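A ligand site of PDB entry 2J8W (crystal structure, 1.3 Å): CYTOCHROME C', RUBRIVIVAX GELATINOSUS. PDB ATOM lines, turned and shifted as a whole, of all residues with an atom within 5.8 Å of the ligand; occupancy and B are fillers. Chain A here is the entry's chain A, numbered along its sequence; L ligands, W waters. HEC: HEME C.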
ATOM      1  N   ILE A   9      28.320 -30.409  -7.308  1.00  0.00           N
ATOM      2  CA  ILE A   9      28.439 -29.338  -6.360  1.00  0.00           C
ATOM      3  C   ILE A   9      27.268 -28.367  -6.484  1.00  0.00           C
ATOM      4  O   ILE A   9      26.660 -27.976  -5.473  1.00  0.00           O
ATOM      5  CB  ILE A   9      29.794 -28.602  -6.546  1.00  0.00           C
ATOM      6  CG1 ILE A   9      30.962 -29.563  -6.217  1.00  0.00           C
ATOM      7  CG2 ILE A   9      29.791 -27.379  -5.666  1.00  0.00           C
ATOM      8  CD1 ILE A   9      32.374 -29.103  -6.650  1.00  0.00           C
ATOM      9  N   ARG A  12      24.039 -30.009  -5.098  1.00  0.00           N
ATOM     10  CA  ARG A  12      23.863 -30.130  -3.660  1.00  0.00           C
ATOM     11  C   ARG A  12      23.673 -28.753  -3.022  1.00  0.00           C
ATOM     12  O   ARG A  12      22.838 -28.585  -2.118  1.00  0.00           O
ATOM     13  CB  ARG A  12      25.025 -30.899  -3.036  1.00  0.00           C
ATOM     14  CG  ARG A  12      26.396 -30.214  -3.007  1.00  0.00           C
ATOM     15  CD  ARG A  12      27.498 -31.254  -3.064  1.00  0.00           C
ATOM     16  NE  ARG A  12      28.810 -30.632  -2.806  1.00  0.00           N
ATOM     17  CZ  ARG A  12      29.953 -31.229  -3.098  1.00  0.00           C
ATOM     18  NH1 ARG A  12      29.944 -32.417  -3.676  1.00  0.00           N
ATOM     19  NH2 ARG A  12      31.137 -30.682  -2.789  1.00  0.00           N
ATOM     20  N   GLN A  13      24.422 -27.752  -3.489  1.00  0.00           N
ATOM     21  CA  GLN A  13      24.193 -26.409  -2.993  1.00  0.00           C
ATOM     22  C   GLN A  13      22.775 -25.956  -3.222  1.00  0.00           C
ATOM     23  O   GLN A  13      22.158 -25.349  -2.332  1.00  0.00           O
ATOM     24  CB  GLN A  13      25.175 -25.434  -3.659  1.00  0.00           C
ATOM     25  CG  GLN A  13      26.641 -25.626  -3.210  1.00  0.00           C
ATOM     26  CD  GLN A  13      27.644 -24.849  -4.028  1.00  0.00           C
ATOM     27  OE1 GLN A  13      27.329 -24.350  -5.126  1.00  0.00           O
ATOM     28  NE2 GLN A  13      28.854 -24.734  -3.509  1.00  0.00           N
ATOM     29  N   SER A  14      22.283 -26.156  -4.430  1.00  0.00           N
ATOM     30  CA  SER A  14      20.918 -25.780  -4.785  1.00  0.00           C
ATOM     31  C   SER A  14      19.914 -26.479  -3.880  1.00  0.00           C
ATOM     32  O   SER A  14      18.965 -25.846  -3.398  1.00  0.00           O
ATOM     33  CB  SER A  14      20.683 -26.138  -6.237  1.00  0.00           C
ATOM     34  OG  SER A  14      21.454 -25.323  -7.119  1.00  0.00           O
ATOM     35  N   PHE A  16      20.372 -27.678  -0.844  1.00  0.00           N
ATOM     36  CA  PHE A  16      20.470 -27.087   0.496  1.00  0.00           C
ATOM     37  C   PHE A  16      19.819 -25.726   0.588  1.00  0.00           C
ATOM     38  O   PHE A  16      19.184 -25.442   1.576  1.00  0.00           O
ATOM     39  CB  PHE A  16      21.919 -27.009   0.957  1.00  0.00           C
ATOM     40  CG  PHE A  16      22.511 -28.331   1.381  1.00  0.00           C
ATOM     41  CD1 PHE A  16      21.903 -29.140   2.312  1.00  0.00           C
ATOM     42  CD2 PHE A  16      23.709 -28.767   0.827  1.00  0.00           C
ATOM     43  CE1 PHE A  16      22.482 -30.370   2.703  1.00  0.00           C
ATOM     44  CE2 PHE A  16      24.317 -29.969   1.225  1.00  0.00           C
ATOM     45  CZ  PHE A  16      23.705 -30.766   2.138  1.00  0.00           C
ATOM     46  N   THR A  17      19.962 -24.906  -0.444  1.00  0.00           N
ATOM     47  CA  THR A  17      19.288 -23.601  -0.446  1.00  0.00           C
ATOM     48  C   THR A  17      17.775 -23.742  -0.362  1.00  0.00           C
ATOM     49  O   THR A  17      17.112 -23.084   0.415  1.00  0.00           O
ATOM     50  CB  THR A  17      19.693 -22.780  -1.671  1.00  0.00           C
ATOM     51  OG1 THR A  17      21.065 -22.427  -1.556  1.00  0.00           O
ATOM     52  CG2 THR A  17      18.873 -21.526  -1.874  1.00  0.00           C
ATOM     53  N   ILE A  19      16.090 -26.373   0.774  1.00  0.00           N
ATOM     54  CA  ILE A  19      15.783 -26.937   2.075  1.00  0.00           C
ATOM     55  C   ILE A  19      15.787 -25.832   3.116  1.00  0.00           C
ATOM     56  O   ILE A  19      14.858 -25.744   3.949  1.00  0.00           O
ATOM     57  CB  ILE A  19      16.813 -28.035   2.442  1.00  0.00           C
ATOM     58  CG1 ILE A  19      16.623 -29.267   1.561  1.00  0.00           C
ATOM     59  CG2 ILE A  19      16.740 -28.377   3.952  1.00  0.00           C
ATOM     60  CD1 ILE A  19      17.803 -30.232   1.614  1.00  0.00           C
ATOM     61  N   ALA A  20      16.828 -24.986   3.111  1.00  0.00           N
ATOM     62  CA  ALA A  20      16.896 -23.943   4.122  1.00  0.00           C
ATOM     63  C   ALA A  20      15.710 -22.999   4.033  1.00  0.00           C
ATOM     64  O   ALA A  20      15.163 -22.574   5.054  1.00  0.00           O
ATOM     65  CB  ALA A  20      18.215 -23.176   3.971  1.00  0.00           C
ATOM     66  N   PHE A  23      12.486 -25.033   5.187  1.00  0.00           N
ATOM     67  CA  PHE A  23      12.623 -25.329   6.604  1.00  0.00           C
ATOM     68  C   PHE A  23      12.472 -24.056   7.437  1.00  0.00           C
ATOM     69  O   PHE A  23      11.842 -24.062   8.479  1.00  0.00           O
ATOM     70  CB  PHE A  23      13.940 -26.029   6.892  1.00  0.00           C
ATOM     71  CG  PHE A  23      14.125 -26.416   8.323  1.00  0.00           C
ATOM     72  CD1 PHE A  23      13.372 -27.379   8.900  1.00  0.00           C
ATOM     73  CD2 PHE A  23      15.099 -25.817   9.103  1.00  0.00           C
ATOM     74  CE1 PHE A  23      13.509 -27.727  10.215  1.00  0.00           C
ATOM     75  CE2 PHE A  23      15.258 -26.164  10.419  1.00  0.00           C
ATOM     76  CZ  PHE A  23      14.484 -27.122  10.965  1.00  0.00           C
ATOM     77  N   VAL A  48      10.435 -30.052   2.420  1.00  0.00           N
ATOM     78  CA  VAL A  48      11.700 -30.346   3.104  1.00  0.00           C
ATOM     79  C   VAL A  48      12.007 -31.823   3.034  1.00  0.00           C
ATOM     80  O   VAL A  48      13.111 -32.230   2.737  1.00  0.00           O
ATOM     81  CB  VAL A  48      11.679 -29.824   4.557  1.00  0.00           C
ATOM     82  CG1 VAL A  48      12.868 -30.354   5.322  1.00  0.00           C
ATOM     83  CG2 VAL A  48      11.641 -28.295   4.579  1.00  0.00           C
ATOM     84  N   LEU A  56      22.632 -35.156  -0.343  1.00  0.00           N
ATOM     85  CA  LEU A  56      23.649 -36.055   0.196  1.00  0.00           C
ATOM     86  C   LEU A  56      23.957 -37.169  -0.802  1.00  0.00           C
ATOM     87  O   LEU A  56      24.911 -37.888  -0.576  1.00  0.00           O
ATOM     88  CB  LEU A  56      23.276 -36.482   1.635  1.00  0.00           C
ATOM     89  CG  LEU A  56      23.180 -35.284   2.608  1.00  0.00           C
ATOM     90  CD1 LEU A  56      22.392 -35.506   3.875  1.00  0.00           C
ATOM     91  CD2 LEU A  56      24.600 -34.787   3.000  1.00  0.00           C
ATOM     92  N   PHE A  59      27.723 -36.021  -3.192  1.00  0.00           N
ATOM     93  CA  PHE A  59      29.073 -35.906  -2.605  1.00  0.00           C
ATOM     94  C   PHE A  59      29.908 -37.141  -2.990  1.00  0.00           C
ATOM     95  O   PHE A  59      30.664 -37.680  -2.176  1.00  0.00           O
ATOM     96  CB  PHE A  59      29.042 -35.754  -1.085  1.00  0.00           C
ATOM     97  CG  PHE A  59      28.514 -34.436  -0.587  1.00  0.00           C
ATOM     98  CD1 PHE A  59      29.368 -33.388  -0.294  1.00  0.00           C
ATOM     99  CD2 PHE A  59      27.148 -34.271  -0.342  1.00  0.00           C
ATOM    100  CE1 PHE A  59      28.879 -32.202   0.209  1.00  0.00           C
ATOM    101  CE2 PHE A  59      26.668 -33.104   0.169  1.00  0.00           C
ATOM    102  CZ  PHE A  59      27.493 -32.053   0.420  1.00  0.00           C
ATOM    103  N   GLY A  68      33.013 -22.873  -5.665  1.00  0.00           N
ATOM    104  CA  GLY A  68      32.578 -22.251  -4.446  1.00  0.00           C
ATOM    105  C   GLY A  68      32.204 -23.256  -3.411  1.00  0.00           C
ATOM    106  O   GLY A  68      31.461 -22.935  -2.461  1.00  0.00           O
ATOM    107  N   THR A  69      32.710 -24.470  -3.562  1.00  0.00           N
ATOM    108  CA  THR A  69      32.350 -25.449  -2.633  1.00  0.00           C
ATOM    109  C   THR A  69      32.837 -25.047  -1.242  1.00  0.00           C
ATOM    110  O   THR A  69      33.962 -24.555  -1.090  1.00  0.00           O
ATOM    111  CB  THR A  69      32.711 -26.907  -2.962  1.00  0.00           C
ATOM    112  OG1 THR A  69      32.085 -27.758  -1.989  1.00  0.00           O
ATOM    113  CG2 THR A  69      34.249 -27.174  -2.914  1.00  0.00           C
ATOM    114  N   GLU A  70      31.969 -25.233  -0.247  1.00  0.00           N
ATOM    115  CA  GLU A  70      32.302 -25.113   1.151  1.00  0.00           C
ATOM    116  C   GLU A  70      32.353 -26.467   1.860  1.00  0.00           C
ATOM    117  O   GLU A  70      32.442 -26.521   3.078  1.00  0.00           O
ATOM    118  CB  GLU A  70      31.274 -24.199   1.840  1.00  0.00           C
ATOM    119  CG  GLU A  70      31.209 -22.789   1.234  1.00  0.00           C
ATOM    120  CD  GLU A  70      30.147 -21.947   1.886  1.00  0.00           C
ATOM    121  OE1 GLU A  70      28.973 -22.415   2.032  1.00  0.00           O
ATOM    122  OE2 GLU A  70      30.494 -20.801   2.246  1.00  0.00           O
ATOM    123  N   ALA A  71      32.354 -27.558   1.097  1.00  0.00           N
ATOM    124  CA  ALA A  71      32.483 -28.892   1.691  1.00  0.00           C
ATOM    125  C   ALA A  71      33.949 -29.059   2.195  1.00  0.00           C
ATOM    126  O   ALA A  71      34.929 -28.927   1.420  1.00  0.00           O
ATOM    127  CB  ALA A  71      32.186 -29.970   0.642  1.00  0.00           C
ATOM    128  N   LYS A  72      34.103 -29.425   3.466  1.00  0.00           N
ATOM    129  CA  LYS A  72      35.456 -29.631   4.019  1.00  0.00           C
ATOM    130  C   LYS A  72      36.020 -30.951   3.522  1.00  0.00           C
ATOM    131  O   LYS A  72      35.290 -31.886   3.207  1.00  0.00           O
ATOM    132  CB  LYS A  72      35.404 -29.645   5.535  1.00  0.00           C
ATOM    133  CG  LYS A  72      35.212 -28.271   6.121  1.00  0.00           C
ATOM    134  CD  LYS A  72      35.023 -28.306   7.627  1.00  0.00           C
ATOM    135  N   VAL A  75      34.642 -34.391   4.610  1.00  0.00           N
ATOM    136  CA  VAL A  75      33.531 -35.099   3.986  1.00  0.00           C
ATOM    137  C   VAL A  75      33.969 -36.425   3.360  1.00  0.00           C
ATOM    138  O   VAL A  75      33.281 -37.434   3.481  1.00  0.00           O
ATOM    139  CB  VAL A  75      32.855 -34.221   2.917  1.00  0.00           C
ATOM    140  CG1 VAL A  75      31.847 -35.033   2.093  1.00  0.00           C
ATOM    141  CG2 VAL A  75      32.119 -33.030   3.563  1.00  0.00           C
ATOM    142  N   PHE A  82      30.731 -38.408   8.221  1.00  0.00           N
ATOM    143  CA  PHE A  82      29.784 -37.735   7.332  1.00  0.00           C
ATOM    144  C   PHE A  82      28.495 -38.546   7.231  1.00  0.00           C
ATOM    145  O   PHE A  82      27.359 -37.974   7.283  1.00  0.00           O
ATOM    146  CB  PHE A  82      30.381 -37.512   5.945  1.00  0.00           C
ATOM    147  CG  PHE A  82      29.579 -36.538   5.104  1.00  0.00           C
ATOM    148  CD1 PHE A  82      29.493 -35.230   5.487  1.00  0.00           C
ATOM    149  CD2 PHE A  82      28.975 -36.941   3.932  1.00  0.00           C
ATOM    150  CE1 PHE A  82      28.747 -34.320   4.738  1.00  0.00           C
ATOM    151  CE2 PHE A  82      28.226 -36.018   3.165  1.00  0.00           C
ATOM    152  CZ  PHE A  82      28.149 -34.732   3.564  1.00  0.00           C
ATOM    153  N   ALA A  85      26.429 -38.225  10.325  1.00  0.00           N
ATOM    154  CA  ALA A  85      25.753 -36.925  10.281  1.00  0.00           C
ATOM    155  C   ALA A  85      24.518 -36.901   9.360  1.00  0.00           C
ATOM    156  O   ALA A  85      23.466 -36.351   9.688  1.00  0.00           O
ATOM    157  CB  ALA A  85      26.760 -35.809   9.900  1.00  0.00           C
ATOM    158  N   ALA A  86      24.671 -37.516   8.211  1.00  0.00           N
ATOM    159  CA  ALA A  86      23.574 -37.661   7.242  1.00  0.00           C
ATOM    160  C   ALA A  86      22.440 -38.485   7.809  1.00  0.00           C
ATOM    161  O   ALA A  86      21.256 -38.119   7.664  1.00  0.00           O
ATOM    162  CB  ALA A  86      24.109 -38.318   5.959  1.00  0.00           C
ATOM    163  N   PHE A  89      20.425 -36.561  10.402  1.00  0.00           N
ATOM    164  CA  PHE A  89      19.528 -35.643   9.699  1.00  0.00           C
ATOM    165  C   PHE A  89      18.323 -36.407   9.141  1.00  0.00           C
ATOM    166  O   PHE A  89      17.179 -35.977   9.307  1.00  0.00           O
ATOM    167  CB  PHE A  89      20.336 -34.989   8.582  1.00  0.00           C
ATOM    168  CG  PHE A  89      19.539 -34.103   7.662  1.00  0.00           C
ATOM    169  CD1 PHE A  89      18.792 -33.032   8.151  1.00  0.00           C
ATOM    170  CD2 PHE A  89      19.525 -34.345   6.305  1.00  0.00           C
ATOM    171  CE1 PHE A  89      18.090 -32.231   7.300  1.00  0.00           C
ATOM    172  CE2 PHE A  89      18.830 -33.491   5.445  1.00  0.00           C
ATOM    173  CZ  PHE A  89      18.128 -32.444   5.951  1.00  0.00           C
ATOM    174  N   THR A 115      15.696 -31.378  13.918  1.00  0.00           N
ATOM    175  CA  THR A 115      16.194 -31.231  12.551  1.00  0.00           C
ATOM    176  C   THR A 115      17.271 -30.163  12.481  1.00  0.00           C
ATOM    177  O   THR A 115      18.347 -30.365  11.928  1.00  0.00           O
ATOM    178  CB  THR A 115      15.036 -30.940  11.576  1.00  0.00           C
ATOM    179  OG1 THR A 115      14.116 -32.024  11.599  1.00  0.00           O
ATOM    180  CG2 THR A 115      15.532 -30.796  10.157  1.00  0.00           C
ATOM    181  N   GLY A 116      17.006 -29.012  13.080  1.00  0.00           N
ATOM    182  CA  GLY A 116      17.978 -27.956  13.124  1.00  0.00           C
ATOM    183  C   GLY A 116      19.274 -28.358  13.787  1.00  0.00           C
ATOM    184  O   GLY A 116      20.361 -27.989  13.310  1.00  0.00           O
ATOM    185  N   ALA A 118      20.524 -31.279  13.683  1.00  0.00           N
ATOM    186  CA  ALA A 118      21.226 -32.116  12.719  1.00  0.00           C
ATOM    187  C   ALA A 118      21.904 -31.263  11.636  1.00  0.00           C
ATOM    188  O   ALA A 118      22.994 -31.610  11.147  1.00  0.00           O
ATOM    189  CB  ALA A 118      20.270 -33.127  12.132  1.00  0.00           C
ATOM    190  N   CYS A 119      21.259 -30.171  11.204  1.00  0.00           N
ATOM    191  CA  CYS A 119      21.913 -29.273  10.252  1.00  0.00           C
ATOM    192  C   CYS A 119      23.231 -28.776  10.843  1.00  0.00           C
ATOM    193  O   CYS A 119      24.288 -28.885  10.227  1.00  0.00           O
ATOM    194  CB  CYS A 119      21.070 -28.044   9.911  1.00  0.00           C
ATOM    195  SG  CYS A 119      19.318 -28.251   9.552  1.00  0.00           S
ATOM    196  N   CYS A 122      26.167 -31.338  11.411  1.00  0.00           N
ATOM    197  CA  CYS A 122      26.914 -31.634  10.201  1.00  0.00           C
ATOM    198  C   CYS A 122      27.778 -30.452   9.827  1.00  0.00           C
ATOM    199  O   CYS A 122      28.978 -30.608   9.566  1.00  0.00           O
ATOM    200  CB  CYS A 122      26.008 -31.996   9.034  1.00  0.00           C
ATOM    201  SG  CYS A 122      27.019 -32.509   7.680  1.00  0.00           S
ATOM    202  N   HIS A 123      27.239 -29.245   9.842  1.00  0.00           N
ATOM    203  CA  HIS A 123      28.022 -28.089   9.408  1.00  0.00           C
ATOM    204  C   HIS A 123      29.270 -27.868  10.257  1.00  0.00           C
ATOM    205  O   HIS A 123      30.358 -27.527   9.733  1.00  0.00           O
ATOM    206  CB  HIS A 123      27.186 -26.817   9.453  1.00  0.00           C
ATOM    207  CG  HIS A 123      26.147 -26.769   8.383  1.00  0.00           C
ATOM    208  ND1 HIS A 123      25.312 -25.710   8.232  1.00  0.00           N
ATOM    209  CD2 HIS A 123      25.875 -27.641   7.387  1.00  0.00           C
ATOM    210  CE1 HIS A 123      24.498 -25.945   7.196  1.00  0.00           C
ATOM    211  NE2 HIS A 123      24.804 -27.107   6.669  1.00  0.00           N
ATOM    212  N   PHE A 126      31.748 -30.453   8.919  1.00  0.00           N
ATOM    213  CA  PHE A 126      31.910 -30.694   7.479  1.00  0.00           C
ATOM    214  C   PHE A 126      31.697 -29.531   6.499  1.00  0.00           C
ATOM    215  O   PHE A 126      31.911 -29.687   5.293  1.00  0.00           O
ATOM    216  CB  PHE A 126      31.016 -31.860   7.048  1.00  0.00           C
ATOM    217  CG  PHE A 126      31.294 -33.104   7.769  1.00  0.00           C
ATOM    218  CD1 PHE A 126      32.445 -33.836   7.470  1.00  0.00           C
ATOM    219  CD2 PHE A 126      30.456 -33.592   8.775  1.00  0.00           C
ATOM    220  CE1 PHE A 126      32.752 -34.994   8.138  1.00  0.00           C
ATOM    221  CE2 PHE A 126      30.757 -34.775   9.428  1.00  0.00           C
ATOM    222  CZ  PHE A 126      31.927 -35.460   9.129  1.00  0.00           C
ATOM    223  N   LYS A 127      31.259 -28.369   6.980  1.00  0.00           N
ATOM    224  CA  LYS A 127      31.052 -27.213   6.132  1.00  0.00           C
ATOM    225  C   LYS A 127      31.920 -26.037   6.615  1.00  0.00           C
ATOM    226  O   LYS A 127      31.942 -25.702   7.807  1.00  0.00           O
ATOM    227  CB  LYS A 127      29.575 -26.798   6.116  1.00  0.00           C
ATOM    228  CG  LYS A 127      29.279 -25.673   5.207  1.00  0.00           C
ATOM    229  CD  LYS A 127      27.841 -25.196   5.379  1.00  0.00           C
ATOM    230  CE  LYS A 127      27.529 -23.997   4.525  1.00  0.00           C
ATOM    231  NZ  LYS A 127      28.212 -22.743   5.015  1.00  0.00           N
HETATM  232 FE   HEC L   1      23.908 -27.970   4.900  1.00  0.00          FE
HETATM  233  CHA HEC L   1      25.693 -26.263   2.520  1.00  0.00           C
HETATM  234  CHB HEC L   1      21.543 -25.559   4.859  1.00  0.00           C
HETATM  235  CHC HEC L   1      21.754 -30.011   6.653  1.00  0.00           C
HETATM  236  CHD HEC L   1      26.226 -30.476   4.858  1.00  0.00           C
HETATM  237  NA  HEC L   1      23.667 -26.272   3.864  1.00  0.00           N
HETATM  238  C1A HEC L   1      24.525 -25.682   2.951  1.00  0.00           C
HETATM  239  C2A HEC L   1      24.020 -24.393   2.545  1.00  0.00           C
HETATM  240  C3A HEC L   1      22.862 -24.198   3.195  1.00  0.00           C
HETATM  241  C4A HEC L   1      22.618 -25.371   4.018  1.00  0.00           C
HETATM  242  CMA HEC L   1      21.900 -23.011   3.094  1.00  0.00           C
HETATM  243  CAA HEC L   1      24.708 -23.445   1.564  1.00  0.00           C
HETATM  244  CBA HEC L   1      24.320 -23.746   0.137  1.00  0.00           C
HETATM  245  CGA HEC L   1      24.936 -22.630  -0.773  1.00  0.00           C
HETATM  246  O1A HEC L   1      25.437 -21.567  -0.289  1.00  0.00           O
HETATM  247  O2A HEC L   1      24.989 -22.731  -2.037  1.00  0.00           O
HETATM  248  NB  HEC L   1      21.968 -27.859   5.588  1.00  0.00           N
HETATM  249  C1B HEC L   1      21.258 -26.691   5.577  1.00  0.00           C
HETATM  250  C2B HEC L   1      20.073 -26.880   6.382  1.00  0.00           C
HETATM  251  C3B HEC L   1      20.122 -28.126   6.867  1.00  0.00           C
HETATM  252  C4B HEC L   1      21.311 -28.766   6.374  1.00  0.00           C
HETATM  253  CMB HEC L   1      18.993 -25.821   6.669  1.00  0.00           C
HETATM  254  CAB HEC L   1      19.106 -28.819   7.762  1.00  0.00           C
HETATM  255  CBB HEC L   1      17.710 -28.698   7.487  1.00  0.00           C
HETATM  256  NC  HEC L   1      23.948 -29.839   5.555  1.00  0.00           N
HETATM  257  C1C HEC L   1      22.997 -30.503   6.305  1.00  0.00           C
HETATM  258  C2C HEC L   1      23.481 -31.790   6.762  1.00  0.00           C
HETATM  259  C3C HEC L   1      24.726 -31.934   6.249  1.00  0.00           C
HETATM  260  C4C HEC L   1      25.056 -30.714   5.521  1.00  0.00           C
HETATM  261  CMC HEC L   1      22.664 -32.777   7.596  1.00  0.00           C
HETATM  262  CAC HEC L   1      25.704 -33.142   6.397  1.00  0.00           C
HETATM  263  CBC HEC L   1      25.214 -34.405   6.691  1.00  0.00           C
HETATM  264  ND  HEC L   1      25.637 -28.321   3.857  1.00  0.00           N
HETATM  265  C1D HEC L   1      26.484 -29.418   4.063  1.00  0.00           C
HETATM  266  C2D HEC L   1      27.686 -29.245   3.275  1.00  0.00           C
HETATM  267  C3D HEC L   1      27.520 -27.994   2.561  1.00  0.00           C
HETATM  268  C4D HEC L   1      26.217 -27.452   2.957  1.00  0.00           C
HETATM  269  CMD HEC L   1      28.863 -30.191   3.210  1.00  0.00           C
HETATM  270  CAD HEC L   1      28.449 -27.380   1.554  1.00  0.00           C
HETATM  271  CBD HEC L   1      28.020 -27.838   0.144  1.00  0.00           C
HETATM  272  CGD HEC L   1      28.995 -27.299  -0.886  1.00  0.00           C
HETATM  273  O1D HEC L   1      29.403 -28.092  -1.763  1.00  0.00           O
HETATM  274  O2D HEC L   1      29.321 -26.058  -0.875  1.00  0.00           O
HETATM  275  O   HOH W   1      24.262 -22.634   5.915  1.00  0.00           O
HETATM  276  O   HOH W   2      22.721 -22.279  -3.614  1.00  0.00           O
HETATM  277  O   HOH W   3      27.815 -24.055   0.308  1.00  0.00           O
HETATM  278  O   HOH W   4      23.577 -19.865   1.409  1.00  0.00           O
HETATM  279  O   HOH W   5      24.948 -19.215  -1.735  1.00  0.00           O
HETATM  280  O   HOH W   6      27.104 -20.838   1.713  1.00  0.00           O
HETATM  281  O   HOH W   7      26.841 -21.294  -3.386  1.00  0.00           O
HETATM  282  O   HOH W   8      28.595 -21.674  -1.686  1.00  0.00           O
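OG1 of Thr 69 is in hydrogen-bond range of NH2 of Arg 12 (3.2 Å). The backbone carbonyl oxygen (O) of Gln 13 sits at hydrogen-bond distance from the side-chain hydroxyl (OG1) of Thr 17, at 3.2 Å. The side-chain amino group of Lys 127 lies within salt-bridge range of the side-chain carboxylate of Glu 70. The backbone NH (N) of Lys 72 lies within hydrogen-bond range of the backbone carbonyl oxygen (O) of Phe 126. The side-chain amide nitrogen of Gln 13 lies within hydrogen-bond range of the backbone carbonyl oxygen of Gly 68, at 3.3 Å. The side-chain hydroxyl (OG1) of Thr 69 is in hydrogen-bond range of the backbone NH (N) of Ala 71 (3.1 Å).
Water W6 bridges the side-chain carboxylate (OE1) of Glu 70 (2.5 Å) and an oxygen (O1A) of the ligand (2.7 Å). Water W3 bridges the side-chain carboxylate (OE1) of Glu 70 (2.6 Å) and an oxygen (O2D) of the ligand (2.8 Å). Water W2 lies within hydrogen-bond range of the side-chain hydroxyl (OG1) of Thr 17 (2.6 Å), an oxygen (O2A) of the ligand (2.8 Å) and the backbone carbonyl oxygen (O) of Gln 13 (3.4 Å). Water W8 bridges the backbone carbonyl oxygen (O) of Gly 68 (3.2 Å) and an oxygen (O1A) of the ligand (3.5 Å).
CG2 of Ile 9 touches O1D of the ligand, at 3.99 Å. CE1 of Phe 16 touches NC of the ligand (3.3 Å). Thr 17 touches the ligand (OG1 to CBA, 3.9 Å). Ile 19 touches the ligand (CG2 to CBB, 3.7 Å). Ala 20 touches the ligand (CB to CMA, 3.8 Å). Leu 56 touches the ligand. CE1 of Phe 59 touches CMD of the ligand (3.6 Å). Ala 71 touches the ligand (N to CGD, 3.9 Å). Phe 82 touches the ligand. C of Ala 85 touches CBC of the ligand, 3.7 Å away. N of Ala 86 touches CBC of the ligand (3.5 Å). CB of Phe 89 touches CMC of the ligand (3.4 Å). Ala 118 touches the ligand. Phe 126 touches the ligand. Lys 127 touches the ligand. Within 4 Å of the ligand: Ile 9, Arg 12, Gln 13, Phe 16, Thr 17, Ile 19, Ala 20, Leu 56, Phe 59, Thr 69, Glu 70, Ala 71, Phe 82, Ala 85, Ala 86, Phe 89, Ala 118, Cys 119, Cys 122, His 123, Phe 126 and Lys 127. Along chain A the residues within 4 Å of the ligand span positions 9 to 127.
An oxygen (O1D) of the ligand lies within salt-bridge range of the guanidinium group (NE) of Arg 12. CAB of the ligand is bonded to SG of Cys 119 (1.9 Å). OG1 of Thr 69 lies within hydrogen-bond range of O1D of the ligand (2.7 Å). A carbon (CAC) of the ligand is covalently linked to the side-chain sulfur (SG) of Cys 122 (1.9 Å). The backbone NH of Glu 70 sits at hydrogen-bond distance from an oxygen (O2D) of the ligand. The side-chain amide nitrogen (NE2) of Gln 13 is in hydrogen-bond range of an oxygen (O2D) of the ligand (3.0 Å). FE of the ligand is bound by NE2 of His 123 (2.2 Å).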
